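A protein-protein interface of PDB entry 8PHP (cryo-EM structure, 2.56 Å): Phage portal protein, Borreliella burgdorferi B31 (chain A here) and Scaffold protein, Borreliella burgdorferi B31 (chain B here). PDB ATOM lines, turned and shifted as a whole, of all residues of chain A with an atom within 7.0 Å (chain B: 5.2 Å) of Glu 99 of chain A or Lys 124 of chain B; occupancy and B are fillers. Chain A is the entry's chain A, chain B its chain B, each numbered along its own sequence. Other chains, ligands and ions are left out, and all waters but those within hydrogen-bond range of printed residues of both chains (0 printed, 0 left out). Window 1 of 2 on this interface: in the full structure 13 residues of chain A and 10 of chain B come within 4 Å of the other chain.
NH2 of Arg 162 of chain B lies close to NH2 of Arg 144 of chain A. The backbone NH (N) of Lys 124 of chain B sits close to the backbone carbonyl oxygen (O) of Ile 98 of chain A, at 3.5 Å. OD1 of Asp 87 of chain A lies within salt-bridge range of NH2 of Arg 162 of chain B, 3.7 Å away. The side-chain carboxylate of Asp 87 of chain A lies within salt-bridge range of the side-chain amino group of Lys 124 of chain B, at 3.2 Å. The backbone carbonyl oxygen (O) of His 93 of chain B lies close to the backbone carbonyl oxygen (O) of Lys 86 of chain A (3.4 Å). The side-chain carboxylate of Asp 91 of chain A is in salt-bridge range of the guanidinium group of Arg 162 of chain B, 3.9 Å away.
The guanidinium group of Arg 144 of chain A is in hydrogen-bond range of the backbone carbonyl oxygen of Asp 91 of chain A (2.7 Å). The backbone NH (N) of Val 83 of chain A is in hydrogen-bond range of the backbone carbonyl oxygen (O) of Arg 144 of chain A (3.0 Å). The guanidinium group (NH1) of Arg 144 of chain A sits at hydrogen-bond distance from the side-chain hydroxyl (OG1) of Thr 85 of chain A. N of Lys 86 of chain A is in hydrogen-bond range of OE2 of Glu 99 of chain A (3.5 Å). The backbone carbonyl oxygen (O) of Tyr 351 of chain A lies within hydrogen-bond range of the backbone NH (N) of Glu 99 of chain A. The side-chain hydroxyl (OG1) of Thr 85 of chain A lies within hydrogen-bond range of the side-chain carboxylate (OD2) of Asp 87 of chain A (2.8 Å).
Among the printed residues, merely in contact across the chains: Lys 86 of chain A with Leu 94 of chain B, Asn 97 of chain A with Arg 123 of chain B, Asn 97 of chain A with Lys 124 of chain B, Asn 97 of chain A with Phe 125 of chain B, Ile 98 of chain A with Arg 123 of chain B, Glu 99 of chain A with His 93 of chain B and Glu 99 of chain A with Lys 124 of chain B.
Glu 99 of chain A touches two residues of chain B. Lys 124 of chain B touches just these residues of chain A: Asp 87 (3.2 Å), Asn 97 (3.7 Å), Ile 98 (3.2 Å) and Glu 99 (3.4 Å). Printed residues of chain B within 4 Å of Lys 86 of chain A: His 93 and Leu 94. Printed residues of chain B within 4 Å of Asn 97 of chain A: Arg 123 (3.4 Å), Lys 124 (3.7 Å) and Phe 125 (3.6 Å). Printed residues of chain A within 4 Å of Leu 94 of chain B: Lys 86. Printed residues of chain B within 4 Å of Ile 98 of chain A: Arg 123 and Lys 124. Of the printed residues of chain B, Asp 87 of chain A touches Lys 124 (3.2 Å) and Arg 162 (3.7 Å). Thr 85 of chain A touches none of the printed residues of chain B. The nearest printed residue of chain B that does not touch Asn 97 of chain A is Val 126 of chain B (4.2 Å).
Of the 10 printed residues of chain B, 6 touch a printed residue of chain A. Printed residues of chain B that touch a printed residue of chain A: His 93, Leu 94, Arg 123, Lys 124, Phe 125 and Arg 162. Printed residues of chain A that touch a printed residue of chain B: Lys 86, Asp 87, Asp 91, Asn 97, Ile 98, Glu 99 and Arg 144. Hydrophobic or aromatic side chains of chain A that line the printed part of chain B: Ile 98. Among the printed residues, 13 pairs touch across the chains.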
ATOM      1  N   VAL A  83      10.601  -7.467  -9.515  1.00  0.00           N
ATOM      2  CA  VAL A  83      11.938  -7.220 -10.036  1.00  0.00           C
ATOM      3  C   VAL A  83      11.870  -5.904 -10.801  1.00  0.00           C
ATOM      4  O   VAL A  83      11.410  -5.858 -11.945  1.00  0.00           O
ATOM      5  CB  VAL A  83      12.425  -8.370 -10.920  1.00  0.00           C
ATOM      6  CG1 VAL A  83      13.904  -8.216 -11.219  1.00  0.00           C
ATOM      7  CG2 VAL A  83      12.150  -9.706 -10.249  1.00  0.00           C
ATOM      8  N   LYS A  84      12.329  -4.827 -10.169  1.00  0.00           N
ATOM      9  CA  LYS A  84      12.224  -3.499 -10.757  1.00  0.00           C
ATOM     10  C   LYS A  84      13.318  -3.288 -11.796  1.00  0.00           C
ATOM     11  O   LYS A  84      14.491  -3.585 -11.549  1.00  0.00           O
ATOM     12  CB  LYS A  84      12.312  -2.428  -9.673  1.00  0.00           C
ATOM     13  CG  LYS A  84      11.430  -2.692  -8.466  1.00  0.00           C
ATOM     14  CD  LYS A  84      11.474  -1.536  -7.481  1.00  0.00           C
ATOM     15  CE  LYS A  84      12.902  -1.104  -7.197  1.00  0.00           C
ATOM     16  NZ  LYS A  84      13.035  -0.483  -5.851  1.00  0.00           N
ATOM     17  N   THR A  85      12.929  -2.775 -12.957  1.00  0.00           N
ATOM     18  CA  THR A  85      13.843  -2.453 -14.043  1.00  0.00           C
ATOM     19  C   THR A  85      13.736  -0.967 -14.373  1.00  0.00           C
ATOM     20  O   THR A  85      12.914  -0.239 -13.812  1.00  0.00           O
ATOM     21  CB  THR A  85      13.550  -3.308 -15.280  1.00  0.00           C
ATOM     22  OG1 THR A  85      12.231  -3.022 -15.761  1.00  0.00           O
ATOM     23  CG2 THR A  85      13.652  -4.788 -14.943  1.00  0.00           C
ATOM     24  N   LYS A  86      14.584  -0.518 -15.298  1.00  0.00           N
ATOM     25  CA  LYS A  86      14.588   0.876 -15.741  1.00  0.00           C
ATOM     26  C   LYS A  86      13.464   1.059 -16.755  1.00  0.00           C
ATOM     27  O   LYS A  86      13.666   1.082 -17.971  1.00  0.00           O
ATOM     28  CB  LYS A  86      15.945   1.253 -16.320  1.00  0.00           C
ATOM     29  CG  LYS A  86      16.097   2.728 -16.659  1.00  0.00           C
ATOM     30  CD  LYS A  86      16.008   3.595 -15.416  1.00  0.00           C
ATOM     31  CE  LYS A  86      16.201   5.063 -15.757  1.00  0.00           C
ATOM     32  NZ  LYS A  86      16.094   5.931 -14.553  1.00  0.00           N
ATOM     33  N   ASP A  87      12.247   1.189 -16.232  1.00  0.00           N
ATOM     34  CA  ASP A  87      11.061   1.310 -17.065  1.00  0.00           C
ATOM     35  C   ASP A  87      10.048   2.198 -16.358  1.00  0.00           C
ATOM     36  O   ASP A  87      10.174   2.498 -15.167  1.00  0.00           O
ATOM     37  CB  ASP A  87      10.453  -0.062 -17.377  1.00  0.00           C
ATOM     38  CG  ASP A  87      11.191  -0.788 -18.484  1.00  0.00           C
ATOM     39  OD1 ASP A  87      11.261  -0.247 -19.607  1.00  0.00           O
ATOM     40  OD2 ASP A  87      11.700  -1.900 -18.232  1.00  0.00           O
ATOM     41  N   ASP A  91       4.999   0.507 -18.330  1.00  0.00           N
ATOM     42  CA  ASP A  91       5.746  -0.535 -19.019  1.00  0.00           C
ATOM     43  C   ASP A  91       5.767  -1.857 -18.263  1.00  0.00           C
ATOM     44  O   ASP A  91       6.248  -2.854 -18.811  1.00  0.00           O
ATOM     45  CB  ASP A  91       7.182  -0.070 -19.273  1.00  0.00           C
ATOM     46  CG  ASP A  91       7.260   1.051 -20.288  1.00  0.00           C
ATOM     47  OD1 ASP A  91       6.201   1.461 -20.807  1.00  0.00           O
ATOM     48  OD2 ASP A  91       8.382   1.525 -20.568  1.00  0.00           O
ATOM     49  N   PRO A  95       6.059  -7.568 -21.417  1.00  0.00           N
ATOM     50  CA  PRO A  95       6.998  -8.605 -20.975  1.00  0.00           C
ATOM     51  C   PRO A  95       8.441  -8.142 -21.113  1.00  0.00           C
ATOM     52  O   PRO A  95       8.750  -7.126 -21.740  1.00  0.00           O
ATOM     53  CB  PRO A  95       6.699  -9.785 -21.908  1.00  0.00           C
ATOM     54  CG  PRO A  95       5.376  -9.459 -22.551  1.00  0.00           C
ATOM     55  CD  PRO A  95       5.332  -7.969 -22.630  1.00  0.00           C
ATOM     56  N   VAL A  96       9.336  -8.916 -20.505  1.00  0.00           N
ATOM     57  CA  VAL A  96      10.767  -8.636 -20.502  1.00  0.00           C
ATOM     58  C   VAL A  96      11.481  -9.769 -21.223  1.00  0.00           C
ATOM     59  O   VAL A  96      11.211 -10.946 -20.959  1.00  0.00           O
ATOM     60  CB  VAL A  96      11.312  -8.475 -19.071  1.00  0.00           C
ATOM     61  CG1 VAL A  96      12.793  -8.134 -19.099  1.00  0.00           C
ATOM     62  CG2 VAL A  96      10.533  -7.412 -18.324  1.00  0.00           C
ATOM     63  N   ASN A  97      12.384  -9.416 -22.138  1.00  0.00           N
ATOM     64  CA  ASN A  97      13.185 -10.418 -22.836  1.00  0.00           C
ATOM     65  C   ASN A  97      14.523 -10.646 -22.134  1.00  0.00           C
ATOM     66  O   ASN A  97      14.788 -11.743 -21.634  1.00  0.00           O
ATOM     67  CB  ASN A  97      13.405  -9.993 -24.291  1.00  0.00           C
ATOM     68  CG  ASN A  97      12.105  -9.828 -25.053  1.00  0.00           C
ATOM     69  OD1 ASN A  97      11.742  -8.723 -25.455  1.00  0.00           O
ATOM     70  ND2 ASN A  97      11.395 -10.931 -25.255  1.00  0.00           N
ATOM     71  N   ILE A  98      15.359  -9.611 -22.074  1.00  0.00           N
ATOM     72  CA  ILE A  98      16.652  -9.661 -21.393  1.00  0.00           C
ATOM     73  C   ILE A  98      16.962  -8.265 -20.875  1.00  0.00           C
ATOM     74  O   ILE A  98      16.984  -7.302 -21.646  1.00  0.00           O
ATOM     75  CB  ILE A  98      17.785 -10.156 -22.319  1.00  0.00           C
ATOM     76  CG1 ILE A  98      17.752 -11.679 -22.467  1.00  0.00           C
ATOM     77  CG2 ILE A  98      19.142  -9.717 -21.791  1.00  0.00           C
ATOM     78  CD1 ILE A  98      18.015 -12.416 -21.173  1.00  0.00           C
ATOM     79  N   GLU A  99      17.210  -8.154 -19.571  1.00  0.00           N
ATOM     80  CA  GLU A  99      17.507  -6.858 -18.976  1.00  0.00           C
ATOM     81  C   GLU A  99      18.093  -7.066 -17.589  1.00  0.00           C
ATOM     82  O   GLU A  99      17.594  -7.890 -16.819  1.00  0.00           O
ATOM     83  CB  GLU A  99      16.248  -5.985 -18.884  1.00  0.00           C
ATOM     84  CG  GLU A  99      16.523  -4.547 -18.476  1.00  0.00           C
ATOM     85  CD  GLU A  99      15.264  -3.704 -18.435  1.00  0.00           C
ATOM     86  OE1 GLU A  99      14.191  -4.213 -18.821  1.00  0.00           O
ATOM     87  OE2 GLU A  99      15.348  -2.530 -18.017  1.00  0.00           O
ATOM     88  N   LEU A 100      19.148  -6.319 -17.283  1.00  0.00           N
ATOM     89  CA  LEU A 100      19.671  -6.311 -15.927  1.00  0.00           C
ATOM     90  C   LEU A 100      18.738  -5.506 -15.024  1.00  0.00           C
ATOM     91  O   LEU A 100      18.348  -4.387 -15.373  1.00  0.00           O
ATOM     92  CB  LEU A 100      21.077  -5.712 -15.898  1.00  0.00           C
ATOM     93  CG  LEU A 100      21.767  -5.558 -14.540  1.00  0.00           C
ATOM     94  CD1 LEU A 100      22.221  -6.908 -14.004  1.00  0.00           C
ATOM     95  CD2 LEU A 100      22.939  -4.599 -14.636  1.00  0.00           C
ATOM     96  N   PRO A 101      18.364  -6.039 -13.866  1.00  0.00           N
ATOM     97  CA  PRO A 101      17.404  -5.343 -13.007  1.00  0.00           C
ATOM     98  C   PRO A 101      18.049  -4.218 -12.211  1.00  0.00           C
ATOM     99  O   PRO A 101      19.267  -4.142 -12.048  1.00  0.00           O
ATOM    100  CB  PRO A 101      16.905  -6.453 -12.079  1.00  0.00           C
ATOM    101  CG  PRO A 101      18.071  -7.365 -11.961  1.00  0.00           C
ATOM    102  CD  PRO A 101      18.756  -7.345 -13.307  1.00  0.00           C
ATOM    103  N   ILE A 102      17.189  -3.332 -11.713  1.00  0.00           N
ATOM    104  CA  ILE A 102      17.639  -2.234 -10.865  1.00  0.00           C
ATOM    105  C   ILE A 102      17.549  -2.592  -9.384  1.00  0.00           C
ATOM    106  O   ILE A 102      18.350  -2.106  -8.581  1.00  0.00           O
ATOM    107  CB  ILE A 102      16.832  -0.960 -11.169  1.00  0.00           C
ATOM    108  CG1 ILE A 102      16.741  -0.731 -12.678  1.00  0.00           C
ATOM    109  CG2 ILE A 102      17.452   0.249 -10.485  1.00  0.00           C
ATOM    110  CD1 ILE A 102      18.076  -0.537 -13.341  1.00  0.00           C
ATOM    111  N   ARG A 144       7.978 -10.482 -14.552  1.00  0.00           N
ATOM    112  CA  ARG A 144       8.741  -9.588 -13.695  1.00  0.00           C
ATOM    113  C   ARG A 144       8.543  -9.888 -12.216  1.00  0.00           C
ATOM    114  O   ARG A 144       8.967  -9.095 -11.371  1.00  0.00           O
ATOM    115  CB  ARG A 144       8.359  -8.134 -13.977  1.00  0.00           C
ATOM    116  CG  ARG A 144       8.243  -7.784 -15.448  1.00  0.00           C
ATOM    117  CD  ARG A 144       7.725  -6.367 -15.627  1.00  0.00           C
ATOM    118  NE  ARG A 144       7.712  -5.955 -17.025  1.00  0.00           N
ATOM    119  CZ  ARG A 144       8.360  -4.901 -17.501  1.00  0.00           C
ATOM    120  NH1 ARG A 144       9.090  -4.126 -16.716  1.00  0.00           N
ATOM    121  NH2 ARG A 144       8.276  -4.620 -18.797  1.00  0.00           N
ATOM    122  N   LEU A 348      14.943 -15.294 -12.971  1.00  0.00           N
ATOM    123  CA  LEU A 348      16.167 -14.503 -12.948  1.00  0.00           C
ATOM    124  C   LEU A 348      17.116 -14.921 -14.065  1.00  0.00           C
ATOM    125  O   LEU A 348      17.718 -14.070 -14.729  1.00  0.00           O
ATOM    126  CB  LEU A 348      16.853 -14.632 -11.588  1.00  0.00           C
ATOM    127  CG  LEU A 348      16.462 -13.608 -10.522  1.00  0.00           C
ATOM    128  CD1 LEU A 348      17.400 -13.697  -9.329  1.00  0.00           C
ATOM    129  CD2 LEU A 348      16.454 -12.202 -11.098  1.00  0.00           C
ATOM    130  N   TYR A 351      14.977 -14.424 -17.823  1.00  0.00           N
ATOM    131  CA  TYR A 351      14.619 -13.076 -18.247  1.00  0.00           C
ATOM    132  C   TYR A 351      15.647 -12.021 -17.870  1.00  0.00           C
ATOM    133  O   TYR A 351      15.738 -10.996 -18.553  1.00  0.00           O
ATOM    134  CB  TYR A 351      13.262 -12.678 -17.656  1.00  0.00           C
ATOM    135  CG  TYR A 351      12.129 -13.596 -18.047  1.00  0.00           C
ATOM    136  CD1 TYR A 351      11.624 -13.594 -19.339  1.00  0.00           C
ATOM    137  CD2 TYR A 351      11.560 -14.462 -17.124  1.00  0.00           C
ATOM    138  CE1 TYR A 351      10.586 -14.430 -19.703  1.00  0.00           C
ATOM    139  CE2 TYR A 351      10.522 -15.301 -17.477  1.00  0.00           C
ATOM    140  CZ  TYR A 351      10.040 -15.282 -18.767  1.00  0.00           C
ATOM    141  OH  TYR A 351       9.006 -16.117 -19.125  1.00  0.00           O
ATOM    142  N   PHE A 352      16.419 -12.233 -16.807  1.00  0.00           N
ATOM    143  CA  PHE A 352      17.352 -11.225 -16.327  1.00  0.00           C
ATOM    144  C   PHE A 352      18.810 -11.654 -16.372  1.00  0.00           C
ATOM    145  O   PHE A 352      19.683 -10.831 -16.078  1.00  0.00           O
ATOM    146  CB  PHE A 352      16.993 -10.812 -14.891  1.00  0.00           C
ATOM    147  CG  PHE A 352      15.587 -10.308 -14.742  1.00  0.00           C
ATOM    148  CD1 PHE A 352      15.285  -8.977 -14.976  1.00  0.00           C
ATOM    149  CD2 PHE A 352      14.564 -11.167 -14.380  1.00  0.00           C
ATOM    150  CE1 PHE A 352      13.991  -8.511 -14.845  1.00  0.00           C
ATOM    151  CE2 PHE A 352      13.268 -10.708 -14.247  1.00  0.00           C
ATOM    152  CZ  PHE A 352      12.981  -9.379 -14.480  1.00  0.00           C
ATOM    153  N   GLY A 353      19.099 -12.901 -16.732  1.00  0.00           N
ATOM    154  CA  GLY A 353      20.480 -13.354 -16.805  1.00  0.00           C
ATOM    155  C   GLY A 353      21.210 -13.313 -15.481  1.00  0.00           C
ATOM    156  O   GLY A 353      22.383 -12.920 -15.433  1.00  0.00           O
ATOM    157  N   LEU A 354      20.542 -13.711 -14.401  1.00  0.00           N
ATOM    158  CA  LEU A 354      21.134 -13.720 -13.074  1.00  0.00           C
ATOM    159  C   LEU A 354      20.883 -15.066 -12.412  1.00  0.00           C
ATOM    160  O   LEU A 354      19.881 -15.732 -12.682  1.00  0.00           O
ATOM    161  CB  LEU A 354      20.567 -12.597 -12.196  1.00  0.00           C
ATOM    162  CG  LEU A 354      21.143 -11.197 -12.416  1.00  0.00           C
ATOM    163  CD1 LEU A 354      20.721 -10.263 -11.294  1.00  0.00           C
ATOM    164  CD2 LEU A 354      22.657 -11.250 -12.531  1.00  0.00           C
ATOM    165  N   HIS B  93      16.756   3.843 -20.673  1.00  0.00           N
ATOM    166  CA  HIS B  93      16.247   2.474 -20.682  1.00  0.00           C
ATOM    167  C   HIS B  93      17.172   1.487 -19.989  1.00  0.00           C
ATOM    168  O   HIS B  93      16.689   0.562 -19.333  1.00  0.00           O
ATOM    169  CB  HIS B  93      15.990   2.018 -22.126  1.00  0.00           C
ATOM    170  CG  HIS B  93      14.853   2.730 -22.787  1.00  0.00           C
ATOM    171  ND1 HIS B  93      13.561   2.666 -22.313  1.00  0.00           N
ATOM    172  CD2 HIS B  93      14.811   3.513 -23.890  1.00  0.00           C
ATOM    173  CE1 HIS B  93      12.772   3.386 -23.090  1.00  0.00           C
ATOM    174  NE2 HIS B  93      13.506   3.909 -24.056  1.00  0.00           N
ATOM    175  N   LEU B  94      18.481   1.651 -20.124  1.00  0.00           N
ATOM    176  CA  LEU B  94      19.431   0.769 -19.468  1.00  0.00           C
ATOM    177  C   LEU B  94      19.742   1.265 -18.058  1.00  0.00           C
ATOM    178  O   LEU B  94      19.434   2.399 -17.685  1.00  0.00           O
ATOM    179  CB  LEU B  94      20.720   0.657 -20.287  1.00  0.00           C
ATOM    180  CG  LEU B  94      20.566   0.115 -21.713  1.00  0.00           C
ATOM    181  CD1 LEU B  94      21.915   0.015 -22.411  1.00  0.00           C
ATOM    182  CD2 LEU B  94      19.860  -1.236 -21.712  1.00  0.00           C
ATOM    183  N   GLU B 120      22.934  -4.312 -25.587  1.00  0.00           N
ATOM    184  CA  GLU B 120      21.973  -4.435 -24.494  1.00  0.00           C
ATOM    185  C   GLU B 120      20.593  -3.947 -24.912  1.00  0.00           C
ATOM    186  O   GLU B 120      19.575  -4.545 -24.542  1.00  0.00           O
ATOM    187  CB  GLU B 120      22.470  -3.663 -23.272  1.00  0.00           C
ATOM    188  CG  GLU B 120      23.772  -4.192 -22.695  1.00  0.00           C
ATOM    189  CD  GLU B 120      23.657  -5.623 -22.205  1.00  0.00           C
ATOM    190  OE1 GLU B 120      22.568  -6.007 -21.726  1.00  0.00           O
ATOM    191  OE2 GLU B 120      24.656  -6.367 -22.307  1.00  0.00           O
ATOM    192  N   LEU B 121      20.537  -2.853 -25.676  1.00  0.00           N
ATOM    193  CA  LEU B 121      19.254  -2.310 -26.110  1.00  0.00           C
ATOM    194  C   LEU B 121      18.508  -3.292 -27.004  1.00  0.00           C
ATOM    195  O   LEU B 121      17.284  -3.430 -26.902  1.00  0.00           O
ATOM    196  CB  LEU B 121      19.467  -0.982 -26.833  1.00  0.00           C
ATOM    197  CG  LEU B 121      19.968   0.165 -25.957  1.00  0.00           C
ATOM    198  CD1 LEU B 121      20.762   1.162 -26.781  1.00  0.00           C
ATOM    199  CD2 LEU B 121      18.808   0.851 -25.255  1.00  0.00           C
ATOM    200  N   VAL B 122      19.229  -3.977 -27.895  1.00  0.00           N
ATOM    201  CA  VAL B 122      18.591  -4.945 -28.783  1.00  0.00           C
ATOM    202  C   VAL B 122      17.964  -6.073 -27.974  1.00  0.00           C
ATOM    203  O   VAL B 122      16.822  -6.479 -28.219  1.00  0.00           O
ATOM    204  CB  VAL B 122      19.603  -5.485 -29.809  1.00  0.00           C
ATOM    205  CG1 VAL B 122      18.951  -6.534 -30.694  1.00  0.00           C
ATOM    206  CG2 VAL B 122      20.158  -4.350 -30.645  1.00  0.00           C
ATOM    207  N   ARG B 123      18.700  -6.590 -26.987  1.00  0.00           N
ATOM    208  CA  ARG B 123      18.167  -7.658 -26.149  1.00  0.00           C
ATOM    209  C   ARG B 123      16.960  -7.184 -25.351  1.00  0.00           C
ATOM    210  O   ARG B 123      15.985  -7.927 -25.184  1.00  0.00           O
ATOM    211  CB  ARG B 123      19.255  -8.186 -25.214  1.00  0.00           C
ATOM    212  CG  ARG B 123      20.476  -8.749 -25.924  1.00  0.00           C
ATOM    213  CD  ARG B 123      21.438  -9.396 -24.938  1.00  0.00           C
ATOM    214  NE  ARG B 123      22.684  -9.811 -25.571  1.00  0.00           N
ATOM    215  CZ  ARG B 123      23.801  -9.094 -25.570  1.00  0.00           C
ATOM    216  NH1 ARG B 123      23.866  -7.917 -24.970  1.00  0.00           N
ATOM    217  NH2 ARG B 123      24.879  -9.573 -26.184  1.00  0.00           N
ATOM    218  N   LYS B 124      17.010  -5.952 -24.842  1.00  0.00           N
ATOM    219  CA  LYS B 124      15.920  -5.445 -24.014  1.00  0.00           C
ATOM    220  C   LYS B 124      14.619  -5.322 -24.800  1.00  0.00           C
ATOM    221  O   LYS B 124      13.554  -5.719 -24.314  1.00  0.00           O
ATOM    222  CB  LYS B 124      16.311  -4.097 -23.408  1.00  0.00           C
ATOM    223  CG  LYS B 124      15.266  -3.500 -22.479  1.00  0.00           C
ATOM    224  CD  LYS B 124      15.645  -2.089 -22.058  1.00  0.00           C
ATOM    225  CE  LYS B 124      14.604  -1.484 -21.128  1.00  0.00           C
ATOM    226  NZ  LYS B 124      13.229  -1.583 -21.688  1.00  0.00           N
ATOM    227  N   PHE B 125      14.680  -4.778 -26.017  1.00  0.00           N
ATOM    228  CA  PHE B 125      13.478  -4.503 -26.800  1.00  0.00           C
ATOM    229  C   PHE B 125      13.221  -5.557 -27.872  1.00  0.00           C
ATOM    230  O   PHE B 125      12.145  -6.161 -27.905  1.00  0.00           O
ATOM    231  CB  PHE B 125      13.581  -3.110 -27.436  1.00  0.00           C
ATOM    232  CG  PHE B 125      13.628  -1.993 -26.435  1.00  0.00           C
ATOM    233  CD1 PHE B 125      12.487  -1.609 -25.749  1.00  0.00           C
ATOM    234  CD2 PHE B 125      14.814  -1.329 -26.175  1.00  0.00           C
ATOM    235  CE1 PHE B 125      12.530  -0.582 -24.825  1.00  0.00           C
ATOM    236  CE2 PHE B 125      14.864  -0.302 -25.254  1.00  0.00           C
ATOM    237  CZ  PHE B 125      13.720   0.071 -24.579  1.00  0.00           C
ATOM    238  N   VAL B 126      14.185  -5.779 -28.760  1.00  0.00           N
ATOM    239  CA  VAL B 126      13.979  -6.732 -29.858  1.00  0.00           C
ATOM    240  C   VAL B 126      13.855  -8.141 -29.289  1.00  0.00           C
ATOM    241  O   VAL B 126      14.704  -8.558 -28.475  1.00  0.00           O
ATOM    242  CB  VAL B 126      15.134  -6.647 -30.872  1.00  0.00           C
ATOM    243  CG1 VAL B 126      14.978  -7.709 -31.945  1.00  0.00           C
ATOM    244  CG2 VAL B 126      15.194  -5.261 -31.493  1.00  0.00           C
ATOM    245  N   ARG B 162       5.933   0.643 -28.465  1.00  0.00           N
ATOM    246  CA  ARG B 162       5.703   0.392 -27.046  1.00  0.00           C
ATOM    247  C   ARG B 162       5.059   1.596 -26.371  1.00  0.00           C
ATOM    248  O   ARG B 162       4.170   1.440 -25.526  1.00  0.00           O
ATOM    249  CB  ARG B 162       7.019   0.030 -26.360  1.00  0.00           C
ATOM    250  CG  ARG B 162       6.869  -0.398 -24.909  1.00  0.00           C
ATOM    251  CD  ARG B 162       8.193  -0.891 -24.344  1.00  0.00           C
ATOM    252  NE  ARG B 162       8.035  -1.488 -23.023  1.00  0.00           N
ATOM    253  CZ  ARG B 162       9.020  -2.039 -22.327  1.00  0.00           C
ATOM    254  NH1 ARG B 162      10.255  -2.088 -22.799  1.00  0.00           N
ATOM    255  NH2 ARG B 162       8.760  -2.555 -21.130  1.00  0.00           N
